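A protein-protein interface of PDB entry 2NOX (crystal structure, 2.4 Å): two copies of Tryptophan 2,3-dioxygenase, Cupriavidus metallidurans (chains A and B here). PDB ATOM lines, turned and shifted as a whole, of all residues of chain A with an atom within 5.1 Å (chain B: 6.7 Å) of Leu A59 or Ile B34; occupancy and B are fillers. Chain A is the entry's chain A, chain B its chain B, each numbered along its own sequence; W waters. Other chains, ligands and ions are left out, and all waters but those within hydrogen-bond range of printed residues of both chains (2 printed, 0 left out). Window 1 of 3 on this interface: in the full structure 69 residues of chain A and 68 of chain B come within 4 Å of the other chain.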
ATOM      1  N   GLN A  33      15.852 -32.667  15.318  1.00  0.00           N
ATOM      2  CA  GLN A  33      14.866 -32.783  14.227  1.00  0.00           C
ATOM      3  C   GLN A  33      14.282 -31.431  13.778  1.00  0.00           C
ATOM      4  O   GLN A  33      14.223 -31.148  12.598  1.00  0.00           O
ATOM      5  CB  GLN A  33      13.677 -33.686  14.612  1.00  0.00           C
ATOM      6  CG  GLN A  33      13.968 -35.078  15.166  1.00  0.00           C
ATOM      7  CD  GLN A  33      12.728 -35.676  15.881  1.00  0.00           C
ATOM      8  OE1 GLN A  33      11.658 -35.863  15.259  1.00  0.00           O
ATOM      9  NE2 GLN A  33      12.865 -35.951  17.200  1.00  0.00           N
ATOM     10  N   ILE A  34      13.829 -30.620  14.733  1.00  0.00           N
ATOM     11  CA  ILE A  34      13.208 -29.302  14.496  1.00  0.00           C
ATOM     12  C   ILE A  34      14.118 -28.457  13.605  1.00  0.00           C
ATOM     13  O   ILE A  34      13.689 -27.861  12.623  1.00  0.00           O
ATOM     14  CB  ILE A  34      12.987 -28.571  15.887  1.00  0.00           C
ATOM     15  CG1 ILE A  34      11.888 -29.248  16.702  1.00  0.00           C
ATOM     16  CG2 ILE A  34      12.715 -27.087  15.765  1.00  0.00           C
ATOM     17  CD1 ILE A  34      10.680 -29.496  15.909  1.00  0.00           C
ATOM     18  N   ALA A  37      15.066 -29.670   9.802  1.00  0.00           N
ATOM     19  CA  ALA A  37      13.913 -29.967   8.976  1.00  0.00           C
ATOM     20  C   ALA A  37      13.744 -28.950   7.873  1.00  0.00           C
ATOM     21  O   ALA A  37      12.740 -28.973   7.163  1.00  0.00           O
ATOM     22  CB  ALA A  37      12.640 -30.076   9.815  1.00  0.00           C
ATOM     23  N   GLN A  38      14.732 -28.073   7.710  1.00  0.00           N
ATOM     24  CA  GLN A  38      14.639 -27.011   6.693  1.00  0.00           C
ATOM     25  C   GLN A  38      15.436 -27.348   5.439  1.00  0.00           C
ATOM     26  O   GLN A  38      16.656 -27.407   5.467  1.00  0.00           O
ATOM     27  CB  GLN A  38      15.104 -25.668   7.270  1.00  0.00           C
ATOM     28  CG  GLN A  38      14.290 -25.175   8.427  1.00  0.00           C
ATOM     29  CD  GLN A  38      14.427 -26.043   9.683  1.00  0.00           C
ATOM     30  OE1 GLN A  38      15.521 -26.469  10.063  1.00  0.00           O
ATOM     31  NE2 GLN A  38      13.315 -26.266  10.349  1.00  0.00           N
ATOM     32  N   HIS A  54       5.669 -21.783   7.350  1.00  0.00           N
ATOM     33  CA  HIS A  54       4.744 -22.892   7.336  1.00  0.00           C
ATOM     34  C   HIS A  54       4.946 -23.758   8.557  1.00  0.00           C
ATOM     35  O   HIS A  54       3.976 -24.167   9.211  1.00  0.00           O
ATOM     36  CB  HIS A  54       4.973 -23.737   6.077  1.00  0.00           C
ATOM     37  CG  HIS A  54       4.247 -23.240   4.871  1.00  0.00           C
ATOM     38  ND1 HIS A  54       4.807 -22.344   3.978  1.00  0.00           N
ATOM     39  CD2 HIS A  54       3.002 -23.503   4.411  1.00  0.00           C
ATOM     40  CE1 HIS A  54       3.940 -22.084   3.015  1.00  0.00           C
ATOM     41  NE2 HIS A  54       2.837 -22.780   3.250  1.00  0.00           N
ATOM     42  N   GLN A  55       6.219 -24.050   8.836  1.00  0.00           N
ATOM     43  CA  GLN A  55       6.627 -24.908   9.945  1.00  0.00           C
ATOM     44  C   GLN A  55       6.142 -24.416  11.317  1.00  0.00           C
ATOM     45  O   GLN A  55       5.592 -25.200  12.108  1.00  0.00           O
ATOM     46  CB  GLN A  55       8.159 -25.136   9.923  1.00  0.00           C
ATOM     47  CG  GLN A  55       8.599 -26.041   8.750  1.00  0.00           C
ATOM     48  CD  GLN A  55      10.063 -26.344   8.707  1.00  0.00           C
ATOM     49  OE1 GLN A  55      10.907 -25.552   9.154  1.00  0.00           O
ATOM     50  NE2 GLN A  55      10.391 -27.496   8.141  1.00  0.00           N
ATOM     51  N   THR A  56       6.342 -23.125  11.582  1.00  0.00           N
ATOM     52  CA  THR A  56       5.885 -22.523  12.835  1.00  0.00           C
ATOM     53  C   THR A  56       4.392 -22.626  12.918  1.00  0.00           C
ATOM     54  O   THR A  56       3.883 -23.027  13.915  1.00  0.00           O
ATOM     55  CB  THR A  56       6.278 -21.009  13.037  1.00  0.00           C
ATOM     56  OG1 THR A  56       5.951 -20.272  11.861  1.00  0.00           O
ATOM     57  CG2 THR A  56       7.739 -20.841  13.380  1.00  0.00           C
ATOM     58  N   THR A  57       3.698 -22.252  11.854  1.00  0.00           N
ATOM     59  CA  THR A  57       2.243 -22.389  11.828  1.00  0.00           C
ATOM     60  C   THR A  57       1.790 -23.825  12.053  1.00  0.00           C
ATOM     61  O   THR A  57       0.846 -24.033  12.776  1.00  0.00           O
ATOM     62  CB  THR A  57       1.604 -21.803  10.545  1.00  0.00           C
ATOM     63  OG1 THR A  57       1.659 -20.379  10.610  1.00  0.00           O
ATOM     64  CG2 THR A  57       0.115 -22.195  10.458  1.00  0.00           C
ATOM     65  N   GLU A  58       2.473 -24.807  11.469  1.00  0.00           N
ATOM     66  CA  GLU A  58       2.073 -26.185  11.655  1.00  0.00           C
ATOM     67  C   GLU A  58       2.277 -26.667  13.082  1.00  0.00           C
ATOM     68  O   GLU A  58       1.427 -27.396  13.660  1.00  0.00           O
ATOM     69  CB  GLU A  58       2.757 -27.059  10.630  1.00  0.00           C
ATOM     70  CG  GLU A  58       2.150 -26.861   9.247  1.00  0.00           C
ATOM     71  CD  GLU A  58       0.893 -27.703   8.981  1.00  0.00           C
ATOM     72  OE1 GLU A  58       0.589 -28.656   9.746  1.00  0.00           O
ATOM     73  OE2 GLU A  58       0.208 -27.427   7.970  1.00  0.00           O
ATOM     74  N   LEU A  59       3.373 -26.201  13.681  1.00  0.00           N
ATOM     75  CA  LEU A  59       3.657 -26.517  15.067  1.00  0.00           C
ATOM     76  C   LEU A  59       2.542 -25.943  15.941  1.00  0.00           C
ATOM     77  O   LEU A  59       1.949 -26.666  16.752  1.00  0.00           O
ATOM     78  CB  LEU A  59       5.009 -25.957  15.484  1.00  0.00           C
ATOM     79  CG  LEU A  59       6.145 -26.968  15.490  1.00  0.00           C
ATOM     80  CD1 LEU A  59       7.386 -26.358  16.071  1.00  0.00           C
ATOM     81  CD2 LEU A  59       5.762 -28.235  16.284  1.00  0.00           C
ATOM     82  N   TRP A  60       2.250 -24.648  15.767  1.00  0.00           N
ATOM     83  CA  TRP A  60       1.143 -24.057  16.522  1.00  0.00           C
ATOM     84  C   TRP A  60      -0.180 -24.782  16.239  1.00  0.00           C
ATOM     85  O   TRP A  60      -0.999 -24.897  17.112  1.00  0.00           O
ATOM     86  CB  TRP A  60       0.999 -22.564  16.244  1.00  0.00           C
ATOM     87  CG  TRP A  60       1.973 -21.601  16.934  1.00  0.00           C
ATOM     88  CD1 TRP A  60       2.728 -20.625  16.318  1.00  0.00           C
ATOM     89  CD2 TRP A  60       2.257 -21.488  18.346  1.00  0.00           C
ATOM     90  NE1 TRP A  60       3.473 -19.934  17.253  1.00  0.00           N
ATOM     91  CE2 TRP A  60       3.201 -20.427  18.501  1.00  0.00           C
ATOM     92  CE3 TRP A  60       1.813 -22.177  19.492  1.00  0.00           C
ATOM     93  CZ2 TRP A  60       3.697 -20.027  19.757  1.00  0.00           C
ATOM     94  CZ3 TRP A  60       2.306 -21.786  20.734  1.00  0.00           C
ATOM     95  CH2 TRP A  60       3.243 -20.710  20.855  1.00  0.00           C
ATOM     96  N   MET A  61      -0.410 -25.272  15.023  1.00  0.00           N
ATOM     97  CA  MET A  61      -1.649 -26.049  14.770  1.00  0.00           C
ATOM     98  C   MET A  61      -1.756 -27.375  15.553  1.00  0.00           C
ATOM     99  O   MET A  61      -2.850 -27.763  16.023  1.00  0.00           O
ATOM    100  CB  MET A  61      -1.846 -26.279  13.286  1.00  0.00           C
ATOM    101  CG  MET A  61      -2.106 -24.971  12.511  1.00  0.00           C
ATOM    102  SD  MET A  61      -2.612 -25.282  10.823  1.00  0.00           S
ATOM    103  CE  MET A  61      -1.274 -26.275  10.304  1.00  0.00           C
ATOM    104  N   LYS A  62      -0.620 -28.055  15.698  1.00  0.00           N
ATOM    105  CA  LYS A  62      -0.552 -29.241  16.545  1.00  0.00           C
ATOM    106  C   LYS A  62      -0.992 -28.902  17.962  1.00  0.00           C
ATOM    107  O   LYS A  62      -1.832 -29.607  18.538  1.00  0.00           O
ATOM    108  CB  LYS A  62       0.857 -29.848  16.561  1.00  0.00           C
ATOM    109  CG  LYS A  62       0.964 -31.036  17.476  1.00  0.00           C
ATOM    110  CD  LYS A  62       1.914 -32.053  16.963  1.00  0.00           C
ATOM    111  CE  LYS A  62       2.443 -32.929  18.117  1.00  0.00           C
ATOM    112  NZ  LYS A  62       3.127 -34.136  17.578  1.00  0.00           N
ATOM    113  N   LEU A  63      -0.433 -27.831  18.519  1.00  0.00           N
ATOM    114  CA  LEU A  63      -0.833 -27.419  19.854  1.00  0.00           C
ATOM    115  C   LEU A  63      -2.309 -27.099  19.931  1.00  0.00           C
ATOM    116  O   LEU A  63      -3.011 -27.523  20.871  1.00  0.00           O
ATOM    117  CB  LEU A  63       0.027 -26.275  20.411  1.00  0.00           C
ATOM    118  CG  LEU A  63      -0.438 -25.891  21.828  1.00  0.00           C
ATOM    119  CD1 LEU A  63      -0.293 -27.033  22.824  1.00  0.00           C
ATOM    120  CD2 LEU A  63       0.198 -24.636  22.363  1.00  0.00           C
ATOM    121  N   GLN A 129      -3.210 -31.543   9.298  1.00  0.00           N
ATOM    122  CA  GLN A 129      -3.591 -30.829  10.548  1.00  0.00           C
ATOM    123  C   GLN A 129      -4.635 -29.760  10.300  1.00  0.00           C
ATOM    124  O   GLN A 129      -5.560 -29.572  11.093  1.00  0.00           O
ATOM    125  CB  GLN A 129      -2.401 -30.178  11.247  1.00  0.00           C
ATOM    126  CG  GLN A 129      -1.407 -31.159  11.808  1.00  0.00           C
ATOM    127  CD  GLN A 129      -0.408 -30.475  12.680  1.00  0.00           C
ATOM    128  OE1 GLN A 129      -0.165 -30.895  13.791  1.00  0.00           O
ATOM    129  NE2 GLN A 129       0.175 -29.393  12.183  1.00  0.00           N
ATOM    130  N   LEU B  29       8.291 -29.646   3.376  1.00  0.00           N
ATOM    131  CA  LEU B  29       8.485 -28.935   4.645  1.00  0.00           C
ATOM    132  C   LEU B  29       9.120 -29.750   5.782  1.00  0.00           C
ATOM    133  O   LEU B  29       9.236 -29.255   6.923  1.00  0.00           O
ATOM    134  CB  LEU B  29       7.161 -28.377   5.138  1.00  0.00           C
ATOM    135  CG  LEU B  29       6.391 -27.366   4.267  1.00  0.00           C
ATOM    136  CD1 LEU B  29       5.048 -27.078   4.878  1.00  0.00           C
ATOM    137  CD2 LEU B  29       7.177 -26.079   4.073  1.00  0.00           C
ATOM    138  N   GLY B  30       9.530 -30.979   5.483  1.00  0.00           N
ATOM    139  CA  GLY B  30       9.987 -31.877   6.528  1.00  0.00           C
ATOM    140  C   GLY B  30       9.066 -32.035   7.731  1.00  0.00           C
ATOM    141  O   GLY B  30       9.537 -32.056   8.859  1.00  0.00           O
ATOM    142  N   LEU B  31       7.767 -32.163   7.494  1.00  0.00           N
ATOM    143  CA  LEU B  31       6.777 -32.222   8.568  1.00  0.00           C
ATOM    144  C   LEU B  31       6.746 -33.519   9.373  1.00  0.00           C
ATOM    145  O   LEU B  31       6.266 -33.522  10.500  1.00  0.00           O
ATOM    146  CB  LEU B  31       5.372 -31.917   8.040  1.00  0.00           C
ATOM    147  CG  LEU B  31       4.997 -30.469   7.737  1.00  0.00           C
ATOM    148  CD1 LEU B  31       3.516 -30.414   7.338  1.00  0.00           C
ATOM    149  CD2 LEU B  31       5.293 -29.514   8.916  1.00  0.00           C
ATOM    150  N   ASP B  32       7.254 -34.615   8.819  1.00  0.00           N
ATOM    151  CA  ASP B  32       7.447 -35.809   9.631  1.00  0.00           C
ATOM    152  C   ASP B  32       8.487 -35.505  10.695  1.00  0.00           C
ATOM    153  O   ASP B  32       8.386 -35.981  11.818  1.00  0.00           O
ATOM    154  CB  ASP B  32       7.878 -37.000   8.787  1.00  0.00           C
ATOM    155  CG  ASP B  32       6.709 -37.836   8.308  1.00  0.00           C
ATOM    156  OD1 ASP B  32       6.702 -39.027   8.668  1.00  0.00           O
ATOM    157  OD2 ASP B  32       5.819 -37.335   7.568  1.00  0.00           O
ATOM    158  N   GLN B  33       9.482 -34.698  10.333  1.00  0.00           N
ATOM    159  CA  GLN B  33      10.518 -34.245  11.267  1.00  0.00           C
ATOM    160  C   GLN B  33       9.992 -33.278  12.326  1.00  0.00           C
ATOM    161  O   GLN B  33      10.281 -33.431  13.502  1.00  0.00           O
ATOM    162  CB  GLN B  33      11.701 -33.600  10.535  1.00  0.00           C
ATOM    163  CG  GLN B  33      12.557 -34.557   9.726  1.00  0.00           C
ATOM    164  CD  GLN B  33      13.671 -33.844   8.964  1.00  0.00           C
ATOM    165  OE1 GLN B  33      14.816 -33.758   9.434  1.00  0.00           O
ATOM    166  NE2 GLN B  33      13.344 -33.333   7.786  1.00  0.00           N
ATOM    167  N   ILE B  34       9.239 -32.275  11.894  1.00  0.00           N
ATOM    168  CA  ILE B  34       8.746 -31.224  12.767  1.00  0.00           C
ATOM    169  C   ILE B  34       7.672 -31.790  13.711  1.00  0.00           C
ATOM    170  O   ILE B  34       7.672 -31.490  14.910  1.00  0.00           O
ATOM    171  CB  ILE B  34       8.092 -30.081  11.903  1.00  0.00           C
ATOM    172  CG1 ILE B  34       9.122 -29.354  11.048  1.00  0.00           C
ATOM    173  CG2 ILE B  34       7.295 -29.098  12.743  1.00  0.00           C
ATOM    174  CD1 ILE B  34      10.092 -28.477  11.831  1.00  0.00           C
ATOM    175  N   LEU B  35       6.766 -32.602  13.150  1.00  0.00           N
ATOM    176  CA  LEU B  35       5.511 -32.979  13.789  1.00  0.00           C
ATOM    177  C   LEU B  35       5.612 -34.282  14.531  1.00  0.00           C
ATOM    178  O   LEU B  35       4.624 -34.855  15.002  1.00  0.00           O
ATOM    179  CB  LEU B  35       4.415 -33.094  12.736  1.00  0.00           C
ATOM    180  CG  LEU B  35       3.398 -31.949  12.594  1.00  0.00           C
ATOM    181  CD1 LEU B  35       3.778 -30.693  13.411  1.00  0.00           C
ATOM    182  CD2 LEU B  35       3.153 -31.640  11.147  1.00  0.00           C
ATOM    183  N   SER B  36       6.819 -34.775  14.636  1.00  0.00           N
ATOM    184  CA  SER B  36       6.973 -35.928  15.460  1.00  0.00           C
ATOM    185  C   SER B  36       8.142 -35.709  16.410  1.00  0.00           C
ATOM    186  O   SER B  36       8.816 -36.640  16.801  1.00  0.00           O
ATOM    187  CB  SER B  36       7.083 -37.193  14.583  1.00  0.00           C
ATOM    188  OG  SER B  36       8.386 -37.375  14.104  1.00  0.00           O
ATOM    189  N   ALA B  37       8.344 -34.451  16.805  1.00  0.00           N
ATOM    190  CA  ALA B  37       9.450 -34.096  17.666  1.00  0.00           C
ATOM    191  C   ALA B  37       8.947 -33.641  19.018  1.00  0.00           C
ATOM    192  O   ALA B  37       9.688 -33.038  19.784  1.00  0.00           O
ATOM    193  CB  ALA B  37      10.273 -33.002  17.022  1.00  0.00           C
ATOM    194  N   GLN B  38       7.679 -33.904  19.303  1.00  0.00           N
ATOM    195  CA  GLN B  38       7.085 -33.492  20.566  1.00  0.00           C
ATOM    196  C   GLN B  38       6.930 -34.698  21.474  1.00  0.00           C
ATOM    197  O   GLN B  38       6.122 -35.554  21.191  1.00  0.00           O
ATOM    198  CB  GLN B  38       5.718 -32.877  20.301  1.00  0.00           C
ATOM    199  CG  GLN B  38       5.782 -31.585  19.528  1.00  0.00           C
ATOM    200  CD  GLN B  38       6.064 -31.803  18.060  1.00  0.00           C
ATOM    201  OE1 GLN B  38       5.460 -32.673  17.400  1.00  0.00           O
ATOM    202  NE2 GLN B  38       6.985 -31.008  17.529  1.00  0.00           N
ATOM    203  N   ILE B  51       6.502 -27.417  25.369  1.00  0.00           N
ATOM    204  CA  ILE B  51       7.381 -27.867  24.301  1.00  0.00           C
ATOM    205  C   ILE B  51       7.240 -26.992  23.064  1.00  0.00           C
ATOM    206  O   ILE B  51       8.244 -26.453  22.586  1.00  0.00           O
ATOM    207  CB  ILE B  51       7.147 -29.381  23.954  1.00  0.00           C
ATOM    208  CG1 ILE B  51       7.574 -30.289  25.131  1.00  0.00           C
ATOM    209  CG2 ILE B  51       7.890 -29.794  22.676  1.00  0.00           C
ATOM    210  CD1 ILE B  51       7.210 -31.815  24.962  1.00  0.00           C
ATOM    211  N   VAL B  52       5.997 -26.829  22.580  1.00  0.00           N
ATOM    212  CA  VAL B  52       5.715 -26.138  21.326  1.00  0.00           C
ATOM    213  C   VAL B  52       6.165 -24.675  21.355  1.00  0.00           C
ATOM    214  O   VAL B  52       6.799 -24.190  20.423  1.00  0.00           O
ATOM    215  CB  VAL B  52       4.216 -26.251  20.886  1.00  0.00           C
ATOM    216  CG1 VAL B  52       3.947 -25.296  19.729  1.00  0.00           C
ATOM    217  CG2 VAL B  52       3.892 -27.698  20.479  1.00  0.00           C
ATOM    218  N   HIS B  54       8.686 -23.456  22.969  1.00  0.00           N
ATOM    219  CA  HIS B  54      10.146 -23.400  22.728  1.00  0.00           C
ATOM    220  C   HIS B  54      10.469 -23.665  21.266  1.00  0.00           C
ATOM    221  O   HIS B  54      11.251 -22.939  20.645  1.00  0.00           O
ATOM    222  CB  HIS B  54      10.897 -24.460  23.546  1.00  0.00           C
ATOM    223  CG  HIS B  54      11.053 -24.127  24.990  1.00  0.00           C
ATOM    224  ND1 HIS B  54      10.107 -24.463  25.935  1.00  0.00           N
ATOM    225  CD2 HIS B  54      12.059 -23.506  25.662  1.00  0.00           C
ATOM    226  CE1 HIS B  54      10.522 -24.065  27.127  1.00  0.00           C
ATOM    227  NE2 HIS B  54      11.704 -23.483  26.991  1.00  0.00           N
ATOM    228  N   GLN B  55       9.901 -24.745  20.740  1.00  0.00           N
ATOM    229  CA  GLN B  55      10.149 -25.154  19.371  1.00  0.00           C
ATOM    230  C   GLN B  55       9.823 -24.082  18.339  1.00  0.00           C
ATOM    231  O   GLN B  55      10.622 -23.844  17.397  1.00  0.00           O
ATOM    232  CB  GLN B  55       9.423 -26.464  19.043  1.00  0.00           C
ATOM    233  CG  GLN B  55       9.794 -27.623  19.985  1.00  0.00           C
ATOM    234  CD  GLN B  55       9.151 -28.915  19.595  1.00  0.00           C
ATOM    235  OE1 GLN B  55       7.969 -28.934  19.215  1.00  0.00           O
ATOM    236  NE2 GLN B  55       9.935 -30.014  19.630  1.00  0.00           N
ATOM    237  N   THR B  56       8.668 -23.430  18.484  1.00  0.00           N
ATOM    238  CA  THR B  56       8.351 -22.333  17.544  1.00  0.00           C
ATOM    239  C   THR B  56       9.361 -21.164  17.660  1.00  0.00           C
ATOM    240  O   THR B  56       9.770 -20.515  16.671  1.00  0.00           O
ATOM    241  CB  THR B  56       6.937 -21.836  17.745  1.00  0.00           C
ATOM    242  OG1 THR B  56       6.744 -21.515  19.137  1.00  0.00           O
ATOM    243  CG2 THR B  56       5.955 -22.916  17.325  1.00  0.00           C
ATOM    244  N   THR B  57       9.800 -20.896  18.871  1.00  0.00           N
ATOM    245  CA  THR B  57      10.751 -19.821  19.056  1.00  0.00           C
ATOM    246  C   THR B  57      12.097 -20.193  18.446  1.00  0.00           C
ATOM    247  O   THR B  57      12.747 -19.374  17.784  1.00  0.00           O
ATOM    248  CB  THR B  57      10.847 -19.426  20.549  1.00  0.00           C
ATOM    249  OG1 THR B  57       9.639 -18.742  20.913  1.00  0.00           O
ATOM    250  CG2 THR B  57      11.995 -18.505  20.785  1.00  0.00           C
ATOM    251  N   LEU B  59      12.544 -22.275  15.856  1.00  0.00           N
ATOM    252  CA  LEU B  59      12.335 -22.134  14.415  1.00  0.00           C
ATOM    253  C   LEU B  59      12.517 -20.684  13.949  1.00  0.00           C
ATOM    254  O   LEU B  59      13.285 -20.417  13.017  1.00  0.00           O
ATOM    255  CB  LEU B  59      10.948 -22.653  14.000  1.00  0.00           C
ATOM    256  CG  LEU B  59      10.881 -24.173  13.863  1.00  0.00           C
ATOM    257  CD1 LEU B  59       9.473 -24.663  13.686  1.00  0.00           C
ATOM    258  CD2 LEU B  59      11.732 -24.568  12.675  1.00  0.00           C
HETATM  259  O   HOH W   1       1.333 -34.986  15.339  1.00  0.00           O
HETATM  260  O   HOH W   2       5.748 -35.944  18.481  1.00  0.00           O
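Of the printed residues of chain B, Ala A37 touches Leu B29 (3.5 Å), Gly B30 (3.8 Å), Gln B33 (3.6 Å) and Ile B34 (3.6 Å).
Thr A57 touches none of the printed residues of chain B.
Of the printed residues of chain B, Leu A59 touches Ile B34, Gln B38, Val B52, Gln B55, Thr B56 and Leu B59.
Printed residues of chain B within 4 Å of Lys A62: Leu B35 (3.1 Å) and Gln B38 (2.8 Å).
Asp B32 touches none of the printed residues of chain A.
Ile B34 touches just these residues of chain A: Ile A34 (3.7 Å), Ala A37 (3.6 Å), Gln A55 (3.7 Å) and Leu A59 (3.7 Å).
Of the printed residues of chain A, Leu B35 touches Lys A62 (3.1 Å) and Gln A129 (3.9 Å).
Printed residues of chain A within 4 Å of Ala B37: Gln A33 and Ile A34.
Of the printed residues of chain A, Val B52 touches Leu A59 (3.8 Å) and Trp A60 (3.8 Å).
The nearest residue of chain A that does not touch Ile B34 is Gln A38 (4.2 Å).
Water W2 lies within hydrogen-bond range of O of Gln B38 (2.8 Å), NZ of Lys A62 (3.3 Å) and N of Ala B37 (3.4 Å).
Water W1 lies within hydrogen-bond range of the side-chain amino group of Lys A62 (3.0 Å) and the backbone carbonyl oxygen of Leu B35 (3.3 Å).
Ile A34 touches Ala B37, and with the chains exchanged Ala A37 touches Ile B34.
Ile A34 touches Leu B59, and with the chains exchanged Leu A59 touches Ile B34.
Thr A56 touches Leu B59, and with the chains exchanged Leu A59 touches Thr B56.
Leu B59 touches its own counterpart, Leu A59.
9 positions are printed for both chains.
Of the 30 pairs that touch across the chains among the printed residues, 18 have their exchanged pair printed and touching as well.
O of Asp B32 sits at hydrogen-bond distance from OG of Ser B36, at 2.7 Å.
OE1 of Glu A58 is in hydrogen-bond range of NE2 of Gln A129 (2.6 Å).
The backbone carbonyl oxygen (O) of Ile B34 is in hydrogen-bond range of the side-chain amide nitrogen (NE2) of Gln B38.
The side-chain amide nitrogen of Gln B55 sits at hydrogen-bond distance from the backbone carbonyl oxygen of Ala B37 (3.0 Å).
The side-chain amide oxygen of Gln A129 lies close to the backbone NH of Lys A62 (3.5 Å).
The backbone carbonyl oxygen (O) of Ile A34 sits at hydrogen-bond distance from the side-chain amide nitrogen (NE2) of Gln A38, 2.8 Å away.
Hydrophobic or aromatic side chains of chain A within 4 Å of the printed part of chain B: Ile A34, Ala A37, His A54, Leu A59 and Trp A60.
Printed residues of chain B that touch a printed residue of chain A: Leu B29, Gly B30, Leu B31, Gln B33, Ile B34, Leu B35, Ser B36, Ala B37, Gln B38, Val B52, Gln B55, Thr B56 and Leu B59.
Hydrophobic or aromatic side chains of chain B within 4 Å of the printed part of chain A: Leu B29, Leu B31, Ile B34, Leu B35, Ala B37, Val B52 and Leu B59.
Along chain B the printed residues that touch a printed residue of chain A span positions 29 to 59.
Among the printed residues, no Asp or Glu carboxylate lies within 4 Å of a Lys or Arg side-chain nitrogen of the other chain.
Among the printed residues, pairs that only touch across the chains: Leu A59 with Gln B38 (3.3 Å), Gln A38 with Leu B59 (3.3 Å), Trp A60 with Thr B56 (3.4 Å), Ala A37 with Leu B29 (3.5 Å), His A54 with Leu B29 (3.6 Å), Leu A59 with Leu B59 (3.6 Å), Ile A34 with Gln B55 (3.6 Å), Leu A59 with Gln B55 (3.6 Å), Ala A37 with Gln B33 (3.6 Å), Ala A37 with Ile B34 (3.6 Å), Gln A33 with Ala B37 (3.6 Å), Leu A59 with Ile B34 (3.7 Å), Gln A55 with Ile B34 (3.7 Å), Leu A59 with Thr B56 (3.7 Å), Ile A34 with Ala B37 (3.7 Å), Ile A34 with Ile B34 (3.7 Å), Thr A56 with Leu B59 (3.7 Å), Gln A55 with Leu B59 (3.7 Å), Trp A60 with Val B52 (3.8 Å), Ala A37 with Gly B30 (3.8 Å), Ile A34 with Leu B59 (3.8 Å), Leu A59 with Val B52 (3.8 Å), Gln A129 with Leu B35 (3.9 Å), Thr A56 with Thr B56 (3.9 Å) and Glu A58 with Leu B31 (3.9 Å).
OE1 of Gln A33 sits close to O of Ser B36, 3.3 Å away.
The side-chain amide nitrogen (NE2) of Gln A55 sits at hydrogen-bond distance from the backbone carbonyl oxygen (O) of Leu B29 (2.4 Å).
OE1 of Gln B38 sits at hydrogen-bond distance from NZ of Lys A62 (2.8 Å).
The backbone carbonyl oxygen of Leu B35 sits at hydrogen-bond distance from the side-chain amino group of Lys A62 (3.1 Å).
The backbone carbonyl oxygen (O) of Gln B33 sits close to the side-chain amide oxygen (OE1) of Gln A33 (3.3 Å).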
